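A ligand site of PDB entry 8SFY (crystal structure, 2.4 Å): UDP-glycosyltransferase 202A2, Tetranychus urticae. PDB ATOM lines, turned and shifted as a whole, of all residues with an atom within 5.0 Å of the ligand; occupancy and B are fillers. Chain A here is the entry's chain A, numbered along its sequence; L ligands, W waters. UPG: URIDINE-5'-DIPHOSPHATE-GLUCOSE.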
ATOM      1  N   PRO A  23       5.757  -5.408  13.822  1.00  0.00           N
ATOM      2  CA  PRO A  23       4.323  -5.602  13.599  1.00  0.00           C
ATOM      3  C   PRO A  23       3.975  -6.196  12.228  1.00  0.00           C
ATOM      4  O   PRO A  23       4.897  -6.528  11.478  1.00  0.00           O
ATOM      5  CB  PRO A  23       3.855  -4.140  13.621  1.00  0.00           C
ATOM      6  CG  PRO A  23       4.983  -3.404  12.886  1.00  0.00           C
ATOM      7  CD  PRO A  23       6.258  -4.168  13.210  1.00  0.00           C
ATOM      8  N   GLY A  24       2.669  -6.298  11.960  1.00  0.00           N
ATOM      9  CA  GLY A  24       2.119  -6.621  10.625  1.00  0.00           C
ATOM     10  C   GLY A  24       1.784  -8.088  10.482  1.00  0.00           C
ATOM     11  O   GLY A  24       0.926  -8.417   9.608  1.00  0.00           O
ATOM     12  N   HIS A  25       2.390  -8.945  11.299  1.00  0.00           N
ATOM     13  CA  HIS A  25       2.259 -10.415  11.141  1.00  0.00           C
ATOM     14  C   HIS A  25       1.004 -10.943  11.868  1.00  0.00           C
ATOM     15  O   HIS A  25       0.707 -12.149  11.764  1.00  0.00           O
ATOM     16  CB  HIS A  25       3.592 -11.065  11.472  1.00  0.00           C
ATOM     17  CG  HIS A  25       4.622 -10.740  10.456  1.00  0.00           C
ATOM     18  ND1 HIS A  25       5.148 -11.691   9.620  1.00  0.00           N
ATOM     19  CD2 HIS A  25       5.171  -9.571  10.077  1.00  0.00           C
ATOM     20  CE1 HIS A  25       6.002 -11.126   8.800  1.00  0.00           C
ATOM     21  NE2 HIS A  25       6.035  -9.841   9.056  1.00  0.00           N
ATOM     22  N   ASN A  27      -2.360  -9.364  11.477  1.00  0.00           N
ATOM     23  CA  ASN A  27      -3.605  -9.019  10.729  1.00  0.00           C
ATOM     24  C   ASN A  27      -4.053 -10.210   9.891  1.00  0.00           C
ATOM     25  O   ASN A  27      -5.281 -10.506   9.867  1.00  0.00           O
ATOM     26  CB  ASN A  27      -3.466  -7.748   9.902  1.00  0.00           C
ATOM     27  CG  ASN A  27      -2.904  -6.596  10.731  1.00  0.00           C
ATOM     28  OD1 ASN A  27      -3.497  -6.191  11.742  1.00  0.00           O
ATOM     29  ND2 ASN A  27      -1.725  -6.107  10.355  1.00  0.00           N
ATOM     30  N   ASP A 140       2.766 -16.823  11.569  1.00  0.00           N
ATOM     31  CA  ASP A 140       3.287 -15.812  10.610  1.00  0.00           C
ATOM     32  C   ASP A 140       4.637 -15.307  11.119  1.00  0.00           C
ATOM     33  O   ASP A 140       4.688 -14.447  12.031  1.00  0.00           O
ATOM     34  CB  ASP A 140       2.287 -14.680  10.336  1.00  0.00           C
ATOM     35  CG  ASP A 140       2.799 -13.785   9.209  1.00  0.00           C
ATOM     36  OD1 ASP A 140       3.966 -14.008   8.804  1.00  0.00           O
ATOM     37  OD2 ASP A 140       2.035 -12.912   8.723  1.00  0.00           O
ATOM     38  N   SER A 160       2.553 -13.126   5.008  1.00  0.00           N
ATOM     39  CA  SER A 160       1.869 -11.843   4.738  1.00  0.00           C
ATOM     40  C   SER A 160       2.850 -10.891   4.042  1.00  0.00           C
ATOM     41  O   SER A 160       2.415  -9.950   3.405  1.00  0.00           O
ATOM     42  CB  SER A 160       1.293 -11.260   5.999  1.00  0.00           C
ATOM     43  OG  SER A 160       2.274 -11.275   7.022  1.00  0.00           O
ATOM     44  N   VAL A 161       4.141 -11.169   4.109  1.00  0.00           N
ATOM     45  CA  VAL A 161       5.135 -10.310   3.400  1.00  0.00           C
ATOM     46  C   VAL A 161       4.916 -10.516   1.898  1.00  0.00           C
ATOM     47  O   VAL A 161       4.267 -11.501   1.500  1.00  0.00           O
ATOM     48  CB  VAL A 161       6.576 -10.588   3.857  1.00  0.00           C
ATOM     49  CG1 VAL A 161       6.778 -10.361   5.340  1.00  0.00           C
ATOM     50  CG2 VAL A 161       7.033 -11.977   3.475  1.00  0.00           C
ATOM     51  N   ASN A 162       5.427  -9.615   1.068  1.00  0.00           N
ATOM     52  CA  ASN A 162       5.476  -9.825  -0.406  1.00  0.00           C
ATOM     53  C   ASN A 162       5.976 -11.244  -0.678  1.00  0.00           C
ATOM     54  O   ASN A 162       7.051 -11.630  -0.212  1.00  0.00           O
ATOM     55  CB  ASN A 162       6.380  -8.779  -1.062  1.00  0.00           C
ATOM     56  CG  ASN A 162       6.538  -9.033  -2.529  1.00  0.00           C
ATOM     57  OD1 ASN A 162       7.270  -9.946  -2.916  1.00  0.00           O
ATOM     58  ND2 ASN A 162       5.795  -8.300  -3.340  1.00  0.00           N
ATOM     59  N   TYR A 274      -5.638   9.805   1.714  1.00  0.00           N
ATOM     60  CA  TYR A 274      -5.183   9.175   2.970  1.00  0.00           C
ATOM     61  C   TYR A 274      -3.667   9.017   2.895  1.00  0.00           C
ATOM     62  O   TYR A 274      -3.178   8.499   1.900  1.00  0.00           O
ATOM     63  CB  TYR A 274      -5.883   7.842   3.183  1.00  0.00           C
ATOM     64  CG  TYR A 274      -5.452   7.063   4.396  1.00  0.00           C
ATOM     65  CD1 TYR A 274      -5.278   7.672   5.629  1.00  0.00           C
ATOM     66  CD2 TYR A 274      -5.280   5.698   4.339  1.00  0.00           C
ATOM     67  CE1 TYR A 274      -4.919   6.957   6.746  1.00  0.00           C
ATOM     68  CE2 TYR A 274      -4.939   4.959   5.461  1.00  0.00           C
ATOM     69  CZ  TYR A 274      -4.758   5.586   6.683  1.00  0.00           C
ATOM     70  OH  TYR A 274      -4.402   4.853   7.787  1.00  0.00           O
ATOM     71  N   SER A 276      -0.465   7.329   5.268  1.00  0.00           N
ATOM     72  CA  SER A 276      -0.080   6.463   6.411  1.00  0.00           C
ATOM     73  C   SER A 276       1.171   5.711   6.018  1.00  0.00           C
ATOM     74  O   SER A 276       1.144   5.005   4.995  1.00  0.00           O
ATOM     75  CB  SER A 276      -1.152   5.490   6.816  1.00  0.00           C
ATOM     76  OG  SER A 276      -0.595   4.443   7.607  1.00  0.00           O
ATOM     77  N   GLY A 278       2.528   3.629   8.144  1.00  0.00           N
ATOM     78  CA  GLY A 278       2.498   2.501   9.088  1.00  0.00           C
ATOM     79  C   GLY A 278       2.916   2.933  10.491  1.00  0.00           C
ATOM     80  O   GLY A 278       3.603   3.953  10.619  1.00  0.00           O
ATOM     81  N   SER A 279       2.491   2.183  11.510  1.00  0.00           N
ATOM     82  CA  SER A 279       2.764   2.414  12.950  1.00  0.00           C
ATOM     83  C   SER A 279       4.263   2.652  13.192  1.00  0.00           C
ATOM     84  O   SER A 279       4.616   3.528  13.998  1.00  0.00           O
ATOM     85  CB  SER A 279       2.284   1.241  13.764  1.00  0.00           C
ATOM     86  OG  SER A 279       2.978   0.049  13.371  1.00  0.00           O
ATOM     87  N   SER A 305      -2.746   9.398   9.134  1.00  0.00           N
ATOM     88  CA  SER A 305      -2.311   8.539  10.273  1.00  0.00           C
ATOM     89  C   SER A 305      -0.953   9.040  10.770  1.00  0.00           C
ATOM     90  O   SER A 305       0.034   8.810  10.089  1.00  0.00           O
ATOM     91  CB  SER A 305      -2.253   7.116   9.904  1.00  0.00           C
ATOM     92  OG  SER A 305      -1.958   6.330  11.039  1.00  0.00           O
ATOM     93  N   LYS A 323      -3.688   9.636  15.635  1.00  0.00           N
ATOM     94  CA  LYS A 323      -2.547   8.700  15.818  1.00  0.00           C
ATOM     95  C   LYS A 323      -2.864   7.386  15.093  1.00  0.00           C
ATOM     96  O   LYS A 323      -2.043   7.000  14.270  1.00  0.00           O
ATOM     97  CB  LYS A 323      -2.230   8.486  17.295  1.00  0.00           C
ATOM     98  CG  LYS A 323      -1.602   9.705  17.958  1.00  0.00           C
ATOM     99  CD  LYS A 323      -1.050   9.454  19.338  1.00  0.00           C
ATOM    100  CE  LYS A 323      -0.250  10.634  19.827  1.00  0.00           C
ATOM    101  NZ  LYS A 323      -0.351  10.797  21.293  1.00  0.00           N
ATOM    102  N   PHE A 324      -4.019   6.782  15.385  1.00  0.00           N
ATOM    103  CA  PHE A 324      -4.536   5.559  14.743  1.00  0.00           C
ATOM    104  C   PHE A 324      -5.896   5.888  14.101  1.00  0.00           C
ATOM    105  O   PHE A 324      -6.747   6.528  14.718  1.00  0.00           O
ATOM    106  CB  PHE A 324      -4.604   4.419  15.772  1.00  0.00           C
ATOM    107  CG  PHE A 324      -4.631   3.021  15.181  1.00  0.00           C
ATOM    108  CD1 PHE A 324      -3.526   2.501  14.530  1.00  0.00           C
ATOM    109  CD2 PHE A 324      -5.776   2.226  15.281  1.00  0.00           C
ATOM    110  CE1 PHE A 324      -3.547   1.223  13.979  1.00  0.00           C
ATOM    111  CE2 PHE A 324      -5.793   0.944  14.743  1.00  0.00           C
ATOM    112  CZ  PHE A 324      -4.682   0.443  14.081  1.00  0.00           C
ATOM    113  N   ILE A 325      -6.065   5.472  12.847  1.00  0.00           N
ATOM    114  CA  ILE A 325      -7.272   5.716  11.992  1.00  0.00           C
ATOM    115  C   ILE A 325      -7.994   4.367  11.825  1.00  0.00           C
ATOM    116  O   ILE A 325      -7.317   3.332  11.816  1.00  0.00           O
ATOM    117  CB  ILE A 325      -6.852   6.299  10.623  1.00  0.00           C
ATOM    118  CG1 ILE A 325      -6.069   7.615  10.745  1.00  0.00           C
ATOM    119  CG2 ILE A 325      -8.021   6.442   9.660  1.00  0.00           C
ATOM    120  CD1 ILE A 325      -6.936   8.844  10.930  1.00  0.00           C
ATOM    121  N   ASN A 326      -9.304   4.376  11.673  1.00  0.00           N
ATOM    122  CA  ASN A 326     -10.046   3.181  11.200  1.00  0.00           C
ATOM    123  C   ASN A 326      -9.782   3.077   9.698  1.00  0.00           C
ATOM    124  O   ASN A 326     -10.622   3.558   8.939  1.00  0.00           O
ATOM    125  CB  ASN A 326     -11.547   3.253  11.537  1.00  0.00           C
ATOM    126  CG  ASN A 326     -12.264   1.969  11.174  1.00  0.00           C
ATOM    127  OD1 ASN A 326     -11.767   1.177  10.378  1.00  0.00           O
ATOM    128  ND2 ASN A 326     -13.441   1.747  11.757  1.00  0.00           N
ATOM    129  N   GLN A 327      -8.635   2.530   9.305  1.00  0.00           N
ATOM    130  CA  GLN A 327      -8.122   2.576   7.905  1.00  0.00           C
ATOM    131  C   GLN A 327      -9.151   1.921   6.956  1.00  0.00           C
ATOM    132  O   GLN A 327      -9.542   2.557   5.969  1.00  0.00           O
ATOM    133  CB  GLN A 327      -6.760   1.895   7.852  1.00  0.00           C
ATOM    134  CG  GLN A 327      -6.200   1.774   6.436  1.00  0.00           C
ATOM    135  CD  GLN A 327      -4.716   1.551   6.425  1.00  0.00           C
ATOM    136  OE1 GLN A 327      -3.955   2.230   7.128  1.00  0.00           O
ATOM    137  NE2 GLN A 327      -4.297   0.602   5.615  1.00  0.00           N
ATOM    138  N   VAL A 328      -9.633   0.742   7.311  1.00  0.00           N
ATOM    139  CA  VAL A 328     -10.547  -0.096   6.475  1.00  0.00           C
ATOM    140  C   VAL A 328     -11.888   0.615   6.275  1.00  0.00           C
ATOM    141  O   VAL A 328     -12.514   0.420   5.216  1.00  0.00           O
ATOM    142  CB  VAL A 328     -10.709  -1.471   7.119  1.00  0.00           C
ATOM    143  CG1 VAL A 328      -9.389  -2.222   7.124  1.00  0.00           C
ATOM    144  CG2 VAL A 328     -11.260  -1.376   8.524  1.00  0.00           C
ATOM    145  N   HIS A 340       3.357   3.202   2.844  1.00  0.00           N
ATOM    146  CA  HIS A 340       4.728   2.672   2.965  1.00  0.00           C
ATOM    147  C   HIS A 340       4.867   1.373   2.165  1.00  0.00           C
ATOM    148  O   HIS A 340       5.986   0.904   2.062  1.00  0.00           O
ATOM    149  CB  HIS A 340       5.152   2.477   4.417  1.00  0.00           C
ATOM    150  CG  HIS A 340       4.473   1.362   5.123  1.00  0.00           C
ATOM    151  ND1 HIS A 340       3.109   1.272   5.210  1.00  0.00           N
ATOM    152  CD2 HIS A 340       4.968   0.339   5.847  1.00  0.00           C
ATOM    153  CE1 HIS A 340       2.778   0.224   5.944  1.00  0.00           C
ATOM    154  NE2 HIS A 340       3.911  -0.369   6.354  1.00  0.00           N
ATOM    155  N   GLY A 341       3.755   0.800   1.678  1.00  0.00           N
ATOM    156  CA  GLY A 341       3.781  -0.411   0.826  1.00  0.00           C
ATOM    157  C   GLY A 341       3.735  -1.691   1.645  1.00  0.00           C
ATOM    158  O   GLY A 341       4.146  -2.732   1.163  1.00  0.00           O
ATOM    159  N   GLY A 342       3.319  -1.624   2.893  1.00  0.00           N
ATOM    160  CA  GLY A 342       3.017  -2.841   3.662  1.00  0.00           C
ATOM    161  C   GLY A 342       1.958  -3.661   2.945  1.00  0.00           C
ATOM    162  O   GLY A 342       1.086  -3.074   2.278  1.00  0.00           O
ATOM    163  N   SER A 343       2.058  -4.973   3.052  1.00  0.00           N
ATOM    164  CA  SER A 343       1.170  -5.927   2.362  1.00  0.00           C
ATOM    165  C   SER A 343      -0.286  -5.697   2.778  1.00  0.00           C
ATOM    166  O   SER A 343      -1.151  -5.762   1.895  1.00  0.00           O
ATOM    167  CB  SER A 343       1.613  -7.339   2.597  1.00  0.00           C
ATOM    168  OG  SER A 343       2.787  -7.613   1.870  1.00  0.00           O
ATOM    169  N   ASN A 344      -0.543  -5.389   4.045  1.00  0.00           N
ATOM    170  CA  ASN A 344      -1.929  -5.294   4.572  1.00  0.00           C
ATOM    171  C   ASN A 344      -2.531  -3.996   4.043  1.00  0.00           C
ATOM    172  O   ASN A 344      -3.676  -4.025   3.581  1.00  0.00           O
ATOM    173  CB  ASN A 344      -1.992  -5.417   6.085  1.00  0.00           C
ATOM    174  CG  ASN A 344      -1.514  -6.770   6.569  1.00  0.00           C
ATOM    175  OD1 ASN A 344      -2.191  -7.762   6.332  1.00  0.00           O
ATOM    176  ND2 ASN A 344      -0.358  -6.813   7.205  1.00  0.00           N
ATOM    177  N   SER A 345      -1.775  -2.905   4.058  1.00  0.00           N
ATOM    178  CA  SER A 345      -2.246  -1.613   3.512  1.00  0.00           C
ATOM    179  C   SER A 345      -2.488  -1.753   2.015  1.00  0.00           C
ATOM    180  O   SER A 345      -3.524  -1.266   1.557  1.00  0.00           O
ATOM    181  CB  SER A 345      -1.314  -0.506   3.867  1.00  0.00           C
ATOM    182  OG  SER A 345      -1.521  -0.101   5.221  1.00  0.00           O
ATOM    183  N   GLU A 348      -5.796  -3.932   1.541  1.00  0.00           N
ATOM    184  CA  GLU A 348      -6.936  -3.099   2.014  1.00  0.00           C
ATOM    185  C   GLU A 348      -7.206  -2.022   0.986  1.00  0.00           C
ATOM    186  O   GLU A 348      -8.361  -1.788   0.655  1.00  0.00           O
ATOM    187  CB  GLU A 348      -6.636  -2.453   3.370  1.00  0.00           C
ATOM    188  CG  GLU A 348      -6.669  -3.440   4.518  1.00  0.00           C
ATOM    189  CD  GLU A 348      -6.008  -2.954   5.798  1.00  0.00           C
ATOM    190  OE1 GLU A 348      -5.844  -1.702   5.957  1.00  0.00           O
ATOM    191  OE2 GLU A 348      -5.630  -3.836   6.651  1.00  0.00           O
ATOM    192  N   PHE A 362      11.128  -0.162   4.204  1.00  0.00           N
ATOM    193  CA  PHE A 362      11.831  -1.325   4.787  1.00  0.00           C
ATOM    194  C   PHE A 362      11.441  -2.635   4.101  1.00  0.00           C
ATOM    195  O   PHE A 362      10.248  -2.865   3.802  1.00  0.00           O
ATOM    196  CB  PHE A 362      11.528  -1.438   6.296  1.00  0.00           C
ATOM    197  CG  PHE A 362      12.484  -2.343   7.017  1.00  0.00           C
ATOM    198  CD1 PHE A 362      13.802  -1.967   7.197  1.00  0.00           C
ATOM    199  CD2 PHE A 362      12.092  -3.598   7.459  1.00  0.00           C
ATOM    200  CE1 PHE A 362      14.709  -2.811   7.828  1.00  0.00           C
ATOM    201  CE2 PHE A 362      12.982  -4.439   8.105  1.00  0.00           C
ATOM    202  CZ  PHE A 362      14.297  -4.045   8.276  1.00  0.00           C
ATOM    203  N   ASP A 364      10.423  -5.972   2.517  1.00  0.00           N
ATOM    204  CA  ASP A 364       9.492  -6.455   1.465  1.00  0.00           C
ATOM    205  C   ASP A 364       8.645  -5.300   0.922  1.00  0.00           C
ATOM    206  O   ASP A 364       7.997  -5.518  -0.108  1.00  0.00           O
ATOM    207  CB  ASP A 364       8.587  -7.563   1.993  1.00  0.00           C
ATOM    208  CG  ASP A 364       7.504  -7.076   2.944  1.00  0.00           C
ATOM    209  OD1 ASP A 364       7.876  -6.374   3.895  1.00  0.00           O
ATOM    210  OD2 ASP A 364       6.292  -7.379   2.711  1.00  0.00           O
ATOM    211  N   GLN A 365       8.608  -4.129   1.579  1.00  0.00           N
ATOM    212  CA  GLN A 365       7.823  -2.952   1.078  1.00  0.00           C
ATOM    213  C   GLN A 365       8.403  -2.495  -0.265  1.00  0.00           C
ATOM    214  O   GLN A 365       7.624  -2.014  -1.143  1.00  0.00           O
ATOM    215  CB  GLN A 365       7.845  -1.785   2.057  1.00  0.00           C
ATOM    216  CG  GLN A 365       7.264  -2.135   3.413  1.00  0.00           C
ATOM    217  CD  GLN A 365       7.691  -1.230   4.532  1.00  0.00           C
ATOM    218  OE1 GLN A 365       8.207  -0.122   4.321  1.00  0.00           O
ATOM    219  NE2 GLN A 365       7.455  -1.712   5.757  1.00  0.00           N
ATOM    220  N   ASN A 368       6.718  -4.584  -2.809  1.00  0.00           N
ATOM    221  CA  ASN A 368       5.288  -4.165  -2.903  1.00  0.00           C
ATOM    222  C   ASN A 368       5.217  -2.868  -3.690  1.00  0.00           C
ATOM    223  O   ASN A 368       4.432  -2.790  -4.634  1.00  0.00           O
ATOM    224  CB  ASN A 368       4.630  -4.030  -1.538  1.00  0.00           C
ATOM    225  CG  ASN A 368       4.222  -5.363  -0.947  1.00  0.00           C
ATOM    226  OD1 ASN A 368       4.063  -6.347  -1.676  1.00  0.00           O
ATOM    227  ND2 ASN A 368       3.992  -5.380   0.356  1.00  0.00           N
HETATM  228  N1  UPG L   1      -3.552   0.600  10.434  1.00  0.00           N
HETATM  229  C2  UPG L   1      -4.759   1.175  10.839  1.00  0.00           C
HETATM  230  N3  UPG L   1      -4.692   2.511  11.118  1.00  0.00           N
HETATM  231  C4  UPG L   1      -3.584   3.330  11.037  1.00  0.00           C
HETATM  232  C5  UPG L   1      -2.380   2.675  10.606  1.00  0.00           C
HETATM  233  C6  UPG L   1      -2.408   1.368  10.325  1.00  0.00           C
HETATM  234  O2  UPG L   1      -5.797   0.538  10.946  1.00  0.00           O
HETATM  235  O4  UPG L   1      -3.683   4.528  11.325  1.00  0.00           O
HETATM  236  C1C UPG L   1      -3.556  -0.844  10.139  1.00  0.00           C
HETATM  237  C2C UPG L   1      -3.862  -1.149   8.676  1.00  0.00           C
HETATM  238  O2C UPG L   1      -5.265  -1.207   8.513  1.00  0.00           O
HETATM  239  C3C UPG L   1      -3.169  -2.513   8.512  1.00  0.00           C
HETATM  240  C4C UPG L   1      -1.926  -2.389   9.419  1.00  0.00           C
HETATM  241  O4C UPG L   1      -2.277  -1.375  10.410  1.00  0.00           O
HETATM  242  O3C UPG L   1      -4.056  -3.552   8.895  1.00  0.00           O
HETATM  243  C5C UPG L   1      -0.646  -2.003   8.714  1.00  0.00           C
HETATM  244  O5C UPG L   1      -0.119  -3.194   8.061  1.00  0.00           O
HETATM  245  PA  UPG L   1       0.945  -3.022   6.874  1.00  0.00           P
HETATM  246  O1A UPG L   1       0.446  -2.002   5.910  1.00  0.00           O
HETATM  247  O2A UPG L   1       1.336  -4.350   6.338  1.00  0.00           O
HETATM  248  O3A UPG L   1       2.147  -2.383   7.696  1.00  0.00           O
HETATM  249  PB  UPG L   1       3.091  -3.055   8.795  1.00  0.00           P
HETATM  250  O1B UPG L   1       2.253  -3.488   9.958  1.00  0.00           O
HETATM  251  O2B UPG L   1       4.249  -2.132   9.029  1.00  0.00           O
HETATM  252  O3B UPG L   1       3.572  -4.331   7.955  1.00  0.00           O
HETATM  253  C1' UPG L   1       4.682  -5.113   8.284  1.00  0.00           C
HETATM  254  C2' UPG L   1       5.838  -4.702   7.399  1.00  0.00           C
HETATM  255  C3' UPG L   1       5.406  -4.861   5.961  1.00  0.00           C
HETATM  256  C4' UPG L   1       4.897  -6.265   5.689  1.00  0.00           C
HETATM  257  C5' UPG L   1       3.848  -6.694   6.730  1.00  0.00           C
HETATM  258  C6' UPG L   1       3.496  -8.168   6.675  1.00  0.00           C
HETATM  259  O2' UPG L   1       6.210  -3.359   7.691  1.00  0.00           O
HETATM  260  O3' UPG L   1       6.507  -4.551   5.120  1.00  0.00           O
HETATM  261  O4' UPG L   1       4.308  -6.299   4.386  1.00  0.00           O
HETATM  262  O5' UPG L   1       4.358  -6.463   8.054  1.00  0.00           O
HETATM  263  O6' UPG L   1       2.131  -8.362   7.036  1.00  0.00           O
HETATM  264  O   HOH W   1      -8.273   0.422  12.259  1.00  0.00           O
HETATM  265  O   HOH W   2       0.813   0.424  10.999  1.00  0.00           O
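The side-chain hydroxyl of Ser 305 lies within hydrogen-bond range of the backbone carbonyl oxygen of Lys 323, at 3.3 Å. The side-chain carboxylate of Asp 364 lies within hydrogen-bond range of the backbone NH of Asn 162, at 2.9 Å. The side-chain amide nitrogen (NE2) of Gln 327 sits at hydrogen-bond distance from the side-chain carboxylate (OE1) of Glu 348 (2.8 Å). O of His 340 sits close to OE1 of Gln 365 (3.3 Å). The side-chain amide oxygen (OE1) of Gln 365 lies within hydrogen-bond range of the backbone NH (N) of Phe 362 (2.9 Å). The side-chain amide nitrogen of Asn 344 is in hydrogen-bond range of the backbone carbonyl oxygen of Gly 24 (3.2 Å). The side-chain hydroxyl (OG) of Ser 343 is in hydrogen-bond range of the backbone NH (N) of Asn 162, 3.4 Å away. OE1 of Gln 327 is in hydrogen-bond range of OH of Tyr 274 (2.7 Å).
Water W1 bridges an oxygen (O2) of the ligand (2.8 Å) and the backbone carbonyl oxygen of Ile 325 (3.1 Å).
The backbone carbonyl oxygen (O) of Pro 23 sits close to an oxygen (O5') of the ligand. CD2 of His 25 touches O5' of the ligand (3.8 Å). Asn 27 touches the ligand (CG to O3C, 3.7 Å). Tyr 274 touches the ligand. Ser 276 touches the ligand. CZ of Phe 324 touches C2 of the ligand, at 3.3 Å. Gln 327 touches the ligand (CD to O2C, 3.5 Å). CA of Gly 342 touches O2A of the ligand, 3.5 Å away. Hydrophobic or aromatic side chains that line the ligand: His 25, Phe 324, Ile 325 and His 340. Within 4 Å of the ligand: Pro 23, Gly 24, His 25, Asn 27, Ser 160, Tyr 274, Ser 276, Ser 305, Phe 324, Ile 325, Gln 327, His 340, Gly 342, Ser 343, Asn 344, Ser 345, Glu 348, Asp 364 and Gln 365.
An oxygen (O4) of the ligand is in hydrogen-bond range of the side-chain hydroxyl (OG) of Ser 305 (2.5 Å). O3' of the ligand sits at hydrogen-bond distance from OD1 of Asp 364, 2.6 Å away. The side-chain carboxylate (OE1) of Glu 348 sits at hydrogen-bond distance from an oxygen (O2C) of the ligand, 2.7 Å away. The backbone NH (N) of Ser 345 lies within hydrogen-bond range of an oxygen (O1A) of the ligand, 3.0 Å away. O1A of the ligand lies within hydrogen-bond range of OG of Ser 345 (2.8 Å). The side-chain amide nitrogen (NE2) of Gln 365 sits at hydrogen-bond distance from an oxygen (O2') of the ligand (2.8 Å). N of Ile 325 lies within hydrogen-bond range of O4 of the ligand, 3.0 Å away. O of Ile 325 sits at hydrogen-bond distance from N3 of the ligand, at 2.8 Å. An oxygen (O1B) of the ligand lies close to the backbone NH (N) of Gly 24 (3.5 Å). The backbone carbonyl oxygen (O) of Gly 24 lies within hydrogen-bond range of an oxygen (O6') of the ligand, at 2.8 Å. The side-chain hydroxyl (OG) of Ser 160 lies within hydrogen-bond range of an oxygen (O6') of the ligand, at 2.9 Å. O4' of the ligand lies within hydrogen-bond range of N of Ser 343, 2.9 Å away. The side-chain hydroxyl (OG) of Ser 343 lies within hydrogen-bond range of an oxygen (O4') of the ligand. The backbone NH (N) of Asn 344 sits at hydrogen-bond distance from an oxygen (O2A) of the ligand, 3.1 Å away. An oxygen (O6') of the ligand sits at hydrogen-bond distance from the side-chain amide nitrogen (ND2) of Asn 344, 2.9 Å away. An oxygen (O3A) of the ligand is in hydrogen-bond range of a ring nitrogen (NE2) of His 340 (3.0 Å).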
